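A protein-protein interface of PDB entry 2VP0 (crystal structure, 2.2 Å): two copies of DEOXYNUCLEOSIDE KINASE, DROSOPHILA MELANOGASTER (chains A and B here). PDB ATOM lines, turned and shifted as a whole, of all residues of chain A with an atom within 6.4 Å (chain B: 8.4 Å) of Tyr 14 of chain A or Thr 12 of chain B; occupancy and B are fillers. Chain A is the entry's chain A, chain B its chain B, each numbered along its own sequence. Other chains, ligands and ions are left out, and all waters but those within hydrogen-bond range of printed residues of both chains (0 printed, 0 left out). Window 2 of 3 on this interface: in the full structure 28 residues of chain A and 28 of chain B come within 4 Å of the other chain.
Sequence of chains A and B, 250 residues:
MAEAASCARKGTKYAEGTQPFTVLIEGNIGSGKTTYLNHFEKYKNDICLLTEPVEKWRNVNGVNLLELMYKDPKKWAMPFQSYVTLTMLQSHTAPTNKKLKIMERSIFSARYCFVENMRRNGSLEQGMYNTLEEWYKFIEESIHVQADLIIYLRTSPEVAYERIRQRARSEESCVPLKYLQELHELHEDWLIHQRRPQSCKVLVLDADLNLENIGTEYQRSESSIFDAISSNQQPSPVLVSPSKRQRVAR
Printed residues of chain B that touch a printed residue of chain A: Thr 12, Tyr 14, Phe 138, Glu 141 and Ser 142. Hydrophobic or aromatic side chains of chain B within 4 Å of the printed part of chain A: Tyr 14 and Phe 138.
Printed residues of chain B within 4 Å of Thr 12 of chain A: Tyr 14. Tyr 14 of chain A touches just these residues of chain B: Thr 12, Glu 141 and Ser 142. No residue of chain B comes within 4 Å of Ala 15 of chain A. Leu 89 of chain A touches none of the printed residues of chain B. Printed residues of chain B within 4 Å of Glu 141 of chain A: Tyr 14. Printed residues of chain B within 4 Å of Ser 142 of chain A: Tyr 14 (3.6 Å). Of the printed residues of chain A, Thr 12 of chain B touches Tyr 14 (3.6 Å). Glu 16 of chain B touches none of the printed residues of chain A. Printed residues of chain A within 4 Å of Ser 142 of chain B: Tyr 14. The nearest residue of chain A that does not touch Thr 12 of chain B is Ala 15 of chain A (4.7 Å). The nearest printed residue of chain B that does not touch Thr 12 of chain A is Ala 15 of chain B (4.7 Å).
O of Thr 12 of chain A touches CD1 of Tyr 14 of chain B (3.6 Å). CD1 of Tyr 14 of chain A touches O of Thr 12 of chain B (3.6 Å). OH of Tyr 14 of chain A touches OE1 of Glu 141 of chain B, at 3.5 Å. CB of Ser 142 of chain B touches CD2 of Tyr 14 of chain A, at 3.6 Å. Phe 138 of chain B touches Thr 93 of chain A (CE1 to OG1, 3.9 Å). O of Glu 141 of chain A touches CE1 of Tyr 14 of chain B, 3.7 Å away. Ser 142 of chain A touches Tyr 14 of chain B (CB to CD2, 3.6 Å).
Thr 12 of chain A touches Tyr 14 of chain B, and with the chains exchanged Tyr 14 of chain A touches Thr 12 of chain B. Tyr 14 of chain A touches Glu 141 of chain B, and with the chains exchanged Glu 141 of chain A touches Tyr 14 of chain B. Tyr 14 of chain A touches Ser 142 of chain B, and with the chains exchanged Ser 142 of chain A touches Tyr 14 of chain B. 9 positions are printed for both chains. Of the 7 pairs that touch across the chains among the printed residues, 6 have their exchanged pair printed and touching as well.
N of Tyr 14 of chain A lies within hydrogen-bond range of O of Ser 142 of chain A (2.9 Å). The backbone carbonyl oxygen (O) of Tyr 14 of chain A is in hydrogen-bond range of the backbone NH (N) of His 144 of chain A (2.8 Å). OG1 of Thr 93 of chain A sits at hydrogen-bond distance from O of Leu 89 of chain A. The backbone NH (N) of Tyr 14 of chain B sits at hydrogen-bond distance from the backbone carbonyl oxygen (O) of Ser 142 of chain B. O of Tyr 14 of chain B is in hydrogen-bond range of N of His 144 of chain B (2.9 Å). O of Phe 138 of chain B sits at hydrogen-bond distance from OG of Ser 142 of chain B, at 3.0 Å.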
ATOM      1  N   THR A  12      -0.924 -10.307  -0.843  1.00  0.00           N
ATOM      2  CA  THR A  12      -2.420 -10.232  -0.855  1.00  0.00           C
ATOM      3  C   THR A  12      -2.938  -9.012  -0.091  1.00  0.00           C
ATOM      4  O   THR A  12      -2.273  -8.496   0.810  1.00  0.00           O
ATOM      5  CB  THR A  12      -3.062 -11.509  -0.285  1.00  0.00           C
ATOM      6  OG1 THR A  12      -2.519 -11.771   1.013  1.00  0.00           O
ATOM      7  CG2 THR A  12      -2.785 -12.704  -1.202  1.00  0.00           C
ATOM      8  N   LYS A  13      -4.137  -8.566  -0.459  1.00  0.00           N
ATOM      9  CA  LYS A  13      -4.746  -7.374   0.113  1.00  0.00           C
ATOM     10  C   LYS A  13      -5.399  -7.701   1.433  1.00  0.00           C
ATOM     11  O   LYS A  13      -5.736  -8.855   1.697  1.00  0.00           O
ATOM     12  CB  LYS A  13      -5.792  -6.810  -0.838  1.00  0.00           C
ATOM     13  CG  LYS A  13      -5.285  -6.554  -2.226  1.00  0.00           C
ATOM     14  CD  LYS A  13      -6.381  -5.986  -3.086  1.00  0.00           C
ATOM     15  CE  LYS A  13      -5.928  -5.854  -4.510  1.00  0.00           C
ATOM     16  NZ  LYS A  13      -7.114  -5.676  -5.374  1.00  0.00           N
ATOM     17  N   TYR A  14      -5.566  -6.687   2.274  1.00  0.00           N
ATOM     18  CA  TYR A  14      -6.302  -6.849   3.510  1.00  0.00           C
ATOM     19  C   TYR A  14      -7.747  -7.290   3.220  1.00  0.00           C
ATOM     20  O   TYR A  14      -8.406  -6.753   2.323  1.00  0.00           O
ATOM     21  CB  TYR A  14      -6.271  -5.555   4.327  1.00  0.00           C
ATOM     22  CG  TYR A  14      -7.054  -5.628   5.618  1.00  0.00           C
ATOM     23  CD1 TYR A  14      -6.628  -6.443   6.668  1.00  0.00           C
ATOM     24  CD2 TYR A  14      -8.222  -4.881   5.788  1.00  0.00           C
ATOM     25  CE1 TYR A  14      -7.343  -6.521   7.854  1.00  0.00           C
ATOM     26  CE2 TYR A  14      -8.939  -4.946   6.965  1.00  0.00           C
ATOM     27  CZ  TYR A  14      -8.494  -5.770   7.995  1.00  0.00           C
ATOM     28  OH  TYR A  14      -9.204  -5.835   9.163  1.00  0.00           O
ATOM     29  N   ALA A  15      -8.200  -8.285   3.987  1.00  0.00           N
ATOM     30  CA  ALA A  15      -9.539  -8.888   3.889  1.00  0.00           C
ATOM     31  C   ALA A  15      -9.787  -9.788   2.661  1.00  0.00           C
ATOM     32  O   ALA A  15     -10.909 -10.263   2.460  1.00  0.00           O
ATOM     33  CB  ALA A  15     -10.645  -7.825   4.032  1.00  0.00           C
ATOM     34  N   GLU A  16      -8.753 -10.026   1.854  1.00  0.00           N
ATOM     35  CA  GLU A  16      -8.863 -10.924   0.701  1.00  0.00           C
ATOM     36  C   GLU A  16      -9.172 -12.346   1.180  1.00  0.00           C
ATOM     37  O   GLU A  16      -8.557 -12.834   2.141  1.00  0.00           O
ATOM     38  CB  GLU A  16      -7.579 -10.900  -0.139  1.00  0.00           C
ATOM     39  CG  GLU A  16      -7.736 -11.517  -1.517  1.00  0.00           C
ATOM     40  CD  GLU A  16      -6.543 -11.268  -2.432  1.00  0.00           C
ATOM     41  OE1 GLU A  16      -5.894 -10.191  -2.321  1.00  0.00           O
ATOM     42  OE2 GLU A  16      -6.267 -12.152  -3.283  1.00  0.00           O
ATOM     43  N   THR A  18     -11.802 -13.345   2.793  1.00  0.00           N
ATOM     44  CA  THR A  18     -12.513 -13.372   4.071  1.00  0.00           C
ATOM     45  C   THR A  18     -13.994 -13.033   3.899  1.00  0.00           C
ATOM     46  O   THR A  18     -14.765 -13.079   4.860  1.00  0.00           O
ATOM     47  CB  THR A  18     -11.885 -12.385   5.104  1.00  0.00           C
ATOM     48  OG1 THR A  18     -12.013 -11.038   4.628  1.00  0.00           O
ATOM     49  CG2 THR A  18     -10.417 -12.686   5.340  1.00  0.00           C
ATOM     50  N   LEU A  89     -15.011   1.457   4.183  1.00  0.00           N
ATOM     51  CA  LEU A  89     -13.923   0.483   4.229  1.00  0.00           C
ATOM     52  C   LEU A  89     -14.029  -0.434   5.455  1.00  0.00           C
ATOM     53  O   LEU A  89     -13.812  -1.634   5.354  1.00  0.00           O
ATOM     54  CB  LEU A  89     -12.592   1.221   4.220  1.00  0.00           C
ATOM     55  CG  LEU A  89     -11.507   0.804   3.242  1.00  0.00           C
ATOM     56  CD1 LEU A  89     -12.071   0.358   1.882  1.00  0.00           C
ATOM     57  CD2 LEU A  89     -10.535   1.969   3.095  1.00  0.00           C
ATOM     58  N   THR A  93     -14.736  -4.514   4.897  1.00  0.00           N
ATOM     59  CA  THR A  93     -13.755  -5.485   5.362  1.00  0.00           C
ATOM     60  C   THR A  93     -14.138  -6.117   6.690  1.00  0.00           C
ATOM     61  O   THR A  93     -13.362  -6.888   7.265  1.00  0.00           O
ATOM     62  CB  THR A  93     -12.346  -4.863   5.478  1.00  0.00           C
ATOM     63  OG1 THR A  93     -12.327  -3.908   6.541  1.00  0.00           O
ATOM     64  CG2 THR A  93     -11.947  -4.178   4.177  1.00  0.00           C
ATOM     65  N   PRO A  95     -15.296  -8.606   9.347  1.00  0.00           N
ATOM     66  CA  PRO A  95     -15.426 -10.066   9.339  1.00  0.00           C
ATOM     67  C   PRO A  95     -16.866 -10.508   9.538  1.00  0.00           C
ATOM     68  O   PRO A  95     -17.650  -9.830  10.197  1.00  0.00           O
ATOM     69  CB  PRO A  95     -14.574 -10.517  10.536  1.00  0.00           C
ATOM     70  CG  PRO A  95     -14.452  -9.321  11.415  1.00  0.00           C
ATOM     71  CD  PRO A  95     -14.538  -8.114  10.513  1.00  0.00           C
ATOM     72  N   GLU A 141      -5.197  -0.966  -4.193  1.00  0.00           N
ATOM     73  CA  GLU A 141      -4.019  -1.833  -4.181  1.00  0.00           C
ATOM     74  C   GLU A 141      -3.901  -2.634  -2.891  1.00  0.00           C
ATOM     75  O   GLU A 141      -3.339  -3.725  -2.878  1.00  0.00           O
ATOM     76  CB  GLU A 141      -2.740  -0.992  -4.337  1.00  0.00           C
ATOM     77  CG  GLU A 141      -2.626  -0.199  -5.640  1.00  0.00           C
ATOM     78  CD  GLU A 141      -1.570   0.924  -5.572  1.00  0.00           C
ATOM     79  OE1 GLU A 141      -0.704   0.911  -4.655  1.00  0.00           O
ATOM     80  OE2 GLU A 141      -1.603   1.821  -6.450  1.00  0.00           O
ATOM     81  N   SER A 142      -4.404  -2.091  -1.794  1.00  0.00           N
ATOM     82  CA  SER A 142      -4.050  -2.619  -0.491  1.00  0.00           C
ATOM     83  C   SER A 142      -5.178  -3.316   0.246  1.00  0.00           C
ATOM     84  O   SER A 142      -4.924  -4.142   1.132  1.00  0.00           O
ATOM     85  CB  SER A 142      -3.498  -1.486   0.383  1.00  0.00           C
ATOM     86  OG  SER A 142      -4.500  -0.533   0.689  1.00  0.00           O
ATOM     87  N   ILE A 143      -6.418  -2.963  -0.097  1.00  0.00           N
ATOM     88  CA  ILE A 143      -7.590  -3.390   0.668  1.00  0.00           C
ATOM     89  C   ILE A 143      -8.586  -4.066  -0.275  1.00  0.00           C
ATOM     90  O   ILE A 143      -8.880  -3.554  -1.360  1.00  0.00           O
ATOM     91  CB  ILE A 143      -8.278  -2.181   1.404  1.00  0.00           C
ATOM     92  CG1 ILE A 143      -7.255  -1.325   2.176  1.00  0.00           C
ATOM     93  CG2 ILE A 143      -9.464  -2.631   2.266  1.00  0.00           C
ATOM     94  CD1 ILE A 143      -6.775  -1.883   3.514  1.00  0.00           C
ATOM     95  N   HIS A 144      -9.106  -5.214   0.148  1.00  0.00           N
ATOM     96  CA  HIS A 144     -10.038  -5.964  -0.680  1.00  0.00           C
ATOM     97  C   HIS A 144     -11.474  -5.525  -0.421  1.00  0.00           C
ATOM     98  O   HIS A 144     -11.962  -5.569   0.717  1.00  0.00           O
ATOM     99  CB  HIS A 144      -9.892  -7.474  -0.476  1.00  0.00           C
ATOM    100  CG  HIS A 144     -10.952  -8.269  -1.171  1.00  0.00           C
ATOM    101  ND1 HIS A 144     -10.865  -8.616  -2.497  1.00  0.00           N
ATOM    102  CD2 HIS A 144     -12.135  -8.759  -0.728  1.00  0.00           C
ATOM    103  CE1 HIS A 144     -11.950  -9.286  -2.847  1.00  0.00           C
ATOM    104  NE2 HIS A 144     -12.735  -9.390  -1.790  1.00  0.00           N
ATOM    105  N   VAL A 145     -12.141  -5.105  -1.492  1.00  0.00           N
ATOM    106  CA  VAL A 145     -13.533  -4.681  -1.428  1.00  0.00           C
ATOM    107  C   VAL A 145     -14.404  -5.688  -2.193  1.00  0.00           C
ATOM    108  O   VAL A 145     -14.431  -5.691  -3.424  1.00  0.00           O
ATOM    109  CB  VAL A 145     -13.702  -3.224  -1.963  1.00  0.00           C
ATOM    110  CG1 VAL A 145     -15.168  -2.791  -1.953  1.00  0.00           C
ATOM    111  CG2 VAL A 145     -12.855  -2.252  -1.143  1.00  0.00           C
ATOM    112  N   THR B  12      -4.839 -10.960   8.904  1.00  0.00           N
ATOM    113  CA  THR B  12      -3.591 -10.813   8.085  1.00  0.00           C
ATOM    114  C   THR B  12      -3.522  -9.449   7.388  1.00  0.00           C
ATOM    115  O   THR B  12      -4.297  -9.159   6.473  1.00  0.00           O
ATOM    116  CB  THR B  12      -3.496 -11.901   7.015  1.00  0.00           C
ATOM    117  OG1 THR B  12      -4.454 -12.932   7.295  1.00  0.00           O
ATOM    118  CG2 THR B  12      -2.082 -12.480   6.962  1.00  0.00           C
ATOM    119  N   LYS B  13      -2.563  -8.630   7.806  1.00  0.00           N
ATOM    120  CA  LYS B  13      -2.472  -7.248   7.351  1.00  0.00           C
ATOM    121  C   LYS B  13      -1.797  -7.149   5.993  1.00  0.00           C
ATOM    122  O   LYS B  13      -1.052  -8.044   5.591  1.00  0.00           O
ATOM    123  CB  LYS B  13      -1.743  -6.404   8.392  1.00  0.00           C
ATOM    124  CG  LYS B  13      -2.352  -6.512   9.785  1.00  0.00           C
ATOM    125  CD  LYS B  13      -1.544  -5.722  10.789  1.00  0.00           C
ATOM    126  CE  LYS B  13      -2.104  -5.872  12.183  1.00  0.00           C
ATOM    127  NZ  LYS B  13      -1.359  -4.994  13.150  1.00  0.00           N
ATOM    128  N   TYR B  14      -2.081  -6.071   5.271  1.00  0.00           N
ATOM    129  CA  TYR B  14      -1.407  -5.806   4.008  1.00  0.00           C
ATOM    130  C   TYR B  14       0.103  -5.603   4.231  1.00  0.00           C
ATOM    131  O   TYR B  14       0.517  -4.937   5.185  1.00  0.00           O
ATOM    132  CB  TYR B  14      -2.029  -4.594   3.316  1.00  0.00           C
ATOM    133  CG  TYR B  14      -1.359  -4.184   2.029  1.00  0.00           C
ATOM    134  CD1 TYR B  14      -1.423  -4.986   0.899  1.00  0.00           C
ATOM    135  CD2 TYR B  14      -0.674  -2.980   1.938  1.00  0.00           C
ATOM    136  CE1 TYR B  14      -0.805  -4.606  -0.292  1.00  0.00           C
ATOM    137  CE2 TYR B  14      -0.060  -2.593   0.759  1.00  0.00           C
ATOM    138  CZ  TYR B  14      -0.131  -3.409  -0.349  1.00  0.00           C
ATOM    139  OH  TYR B  14       0.477  -3.014  -1.519  1.00  0.00           O
ATOM    140  N   ALA B  15       0.897  -6.204   3.346  1.00  0.00           N
ATOM    141  CA  ALA B  15       2.364  -6.140   3.374  1.00  0.00           C
ATOM    142  C   ALA B  15       3.010  -6.941   4.510  1.00  0.00           C
ATOM    143  O   ALA B  15       4.240  -6.965   4.626  1.00  0.00           O
ATOM    144  CB  ALA B  15       2.859  -4.672   3.375  1.00  0.00           C
ATOM    145  N   GLU B  16       2.188  -7.593   5.337  1.00  0.00           N
ATOM    146  CA  GLU B  16       2.681  -8.420   6.450  1.00  0.00           C
ATOM    147  C   GLU B  16       3.582  -9.574   5.981  1.00  0.00           C
ATOM    148  O   GLU B  16       3.184 -10.382   5.143  1.00  0.00           O
ATOM    149  CB  GLU B  16       1.520  -8.948   7.297  1.00  0.00           C
ATOM    150  CG  GLU B  16       1.946  -9.757   8.507  1.00  0.00           C
ATOM    151  CD  GLU B  16       1.006  -9.595   9.680  1.00  0.00           C
ATOM    152  OE1 GLU B  16      -0.136 -10.107   9.624  1.00  0.00           O
ATOM    153  OE2 GLU B  16       1.415  -8.953  10.669  1.00  0.00           O
ATOM    154  N   GLY B  17       4.802  -9.611   6.521  1.00  0.00           N
ATOM    155  CA  GLY B  17       5.788 -10.632   6.187  1.00  0.00           C
ATOM    156  C   GLY B  17       6.522 -10.408   4.874  1.00  0.00           C
ATOM    157  O   GLY B  17       7.209 -11.305   4.392  1.00  0.00           O
ATOM    158  N   PHE B 138      -7.507   2.397  12.115  1.00  0.00           N
ATOM    159  CA  PHE B 138      -7.829   1.409  11.095  1.00  0.00           C
ATOM    160  C   PHE B 138      -6.559   0.901  10.427  1.00  0.00           C
ATOM    161  O   PHE B 138      -6.431  -0.298  10.174  1.00  0.00           O
ATOM    162  CB  PHE B 138      -8.795   1.967  10.043  1.00  0.00           C
ATOM    163  CG  PHE B 138      -9.100   0.988   8.928  1.00  0.00           C
ATOM    164  CD1 PHE B 138      -9.893  -0.131   9.163  1.00  0.00           C
ATOM    165  CD2 PHE B 138      -8.574   1.176   7.657  1.00  0.00           C
ATOM    166  CE1 PHE B 138     -10.163  -1.046   8.141  1.00  0.00           C
ATOM    167  CE2 PHE B 138      -8.840   0.268   6.625  1.00  0.00           C
ATOM    168  CZ  PHE B 138      -9.631  -0.847   6.872  1.00  0.00           C
ATOM    169  N   ILE B 139      -5.633   1.818  10.142  1.00  0.00           N
ATOM    170  CA  ILE B 139      -4.349   1.484   9.519  1.00  0.00           C
ATOM    171  C   ILE B 139      -3.569   0.461  10.367  1.00  0.00           C
ATOM    172  O   ILE B 139      -3.020  -0.503   9.846  1.00  0.00           O
ATOM    173  CB  ILE B 139      -3.498   2.773   9.268  1.00  0.00           C
ATOM    174  CG1 ILE B 139      -4.141   3.638   8.175  1.00  0.00           C
ATOM    175  CG2 ILE B 139      -2.024   2.433   8.948  1.00  0.00           C
ATOM    176  CD1 ILE B 139      -3.651   5.077   8.143  1.00  0.00           C
ATOM    177  N   GLU B 140      -3.554   0.680  11.678  1.00  0.00           N
ATOM    178  CA  GLU B 140      -2.940  -0.241  12.628  1.00  0.00           C
ATOM    179  C   GLU B 140      -3.527  -1.660  12.571  1.00  0.00           C
ATOM    180  O   GLU B 140      -2.791  -2.630  12.708  1.00  0.00           O
ATOM    181  CB  GLU B 140      -3.050   0.328  14.040  1.00  0.00           C
ATOM    182  CG  GLU B 140      -2.040  -0.246  15.026  1.00  0.00           C
ATOM    183  CD  GLU B 140      -2.111   0.437  16.381  1.00  0.00           C
ATOM    184  OE1 GLU B 140      -2.094   1.700  16.418  1.00  0.00           O
ATOM    185  OE2 GLU B 140      -2.191  -0.290  17.408  1.00  0.00           O
ATOM    186  N   GLU B 141      -4.833  -1.792  12.352  1.00  0.00           N
ATOM    187  CA  GLU B 141      -5.434  -3.133  12.290  1.00  0.00           C
ATOM    188  C   GLU B 141      -5.330  -3.787  10.906  1.00  0.00           C
ATOM    189  O   GLU B 141      -5.386  -5.008  10.794  1.00  0.00           O
ATOM    190  CB  GLU B 141      -6.886  -3.155  12.829  1.00  0.00           C
ATOM    191  CG  GLU B 141      -7.965  -2.676  11.847  1.00  0.00           C
ATOM    192  CD  GLU B 141      -9.382  -3.159  12.197  1.00  0.00           C
ATOM    193  OE1 GLU B 141      -9.595  -4.392  12.345  1.00  0.00           O
ATOM    194  OE2 GLU B 141     -10.289  -2.295  12.303  1.00  0.00           O
ATOM    195  N   SER B 142      -5.133  -2.975   9.869  1.00  0.00           N
ATOM    196  CA  SER B 142      -5.243  -3.431   8.482  1.00  0.00           C
ATOM    197  C   SER B 142      -3.942  -3.457   7.674  1.00  0.00           C
ATOM    198  O   SER B 142      -3.840  -4.170   6.670  1.00  0.00           O
ATOM    199  CB  SER B 142      -6.280  -2.575   7.734  1.00  0.00           C
ATOM    200  OG  SER B 142      -5.794  -1.263   7.446  1.00  0.00           O
ATOM    201  N   ILE B 143      -2.968  -2.650   8.076  1.00  0.00           N
ATOM    202  CA  ILE B 143      -1.742  -2.495   7.302  1.00  0.00           C
ATOM    203  C   ILE B 143      -0.524  -2.708   8.203  1.00  0.00           C
ATOM    204  O   ILE B 143      -0.435  -2.120   9.279  1.00  0.00           O
ATOM    205  CB  ILE B 143      -1.690  -1.109   6.610  1.00  0.00           C
ATOM    206  CG1 ILE B 143      -2.818  -0.990   5.573  1.00  0.00           C
ATOM    207  CG2 ILE B 143      -0.320  -0.857   5.978  1.00  0.00           C
ATOM    208  CD1 ILE B 143      -2.872   0.329   4.871  1.00  0.00           C
ATOM    209  N   HIS B 144       0.394  -3.570   7.762  1.00  0.00           N
ATOM    210  CA  HIS B 144       1.603  -3.883   8.532  1.00  0.00           C
ATOM    211  C   HIS B 144       2.650  -2.784   8.363  1.00  0.00           C
ATOM    212  O   HIS B 144       3.059  -2.479   7.246  1.00  0.00           O
ATOM    213  CB  HIS B 144       2.185  -5.252   8.129  1.00  0.00           C
ATOM    214  CG  HIS B 144       3.498  -5.564   8.783  1.00  0.00           C
ATOM    215  ND1 HIS B 144       3.594  -5.991  10.090  1.00  0.00           N
ATOM    216  CD2 HIS B 144       4.769  -5.485   8.319  1.00  0.00           C
ATOM    217  CE1 HIS B 144       4.868  -6.159  10.405  1.00  0.00           C
ATOM    218  NE2 HIS B 144       5.602  -5.863   9.346  1.00  0.00           N
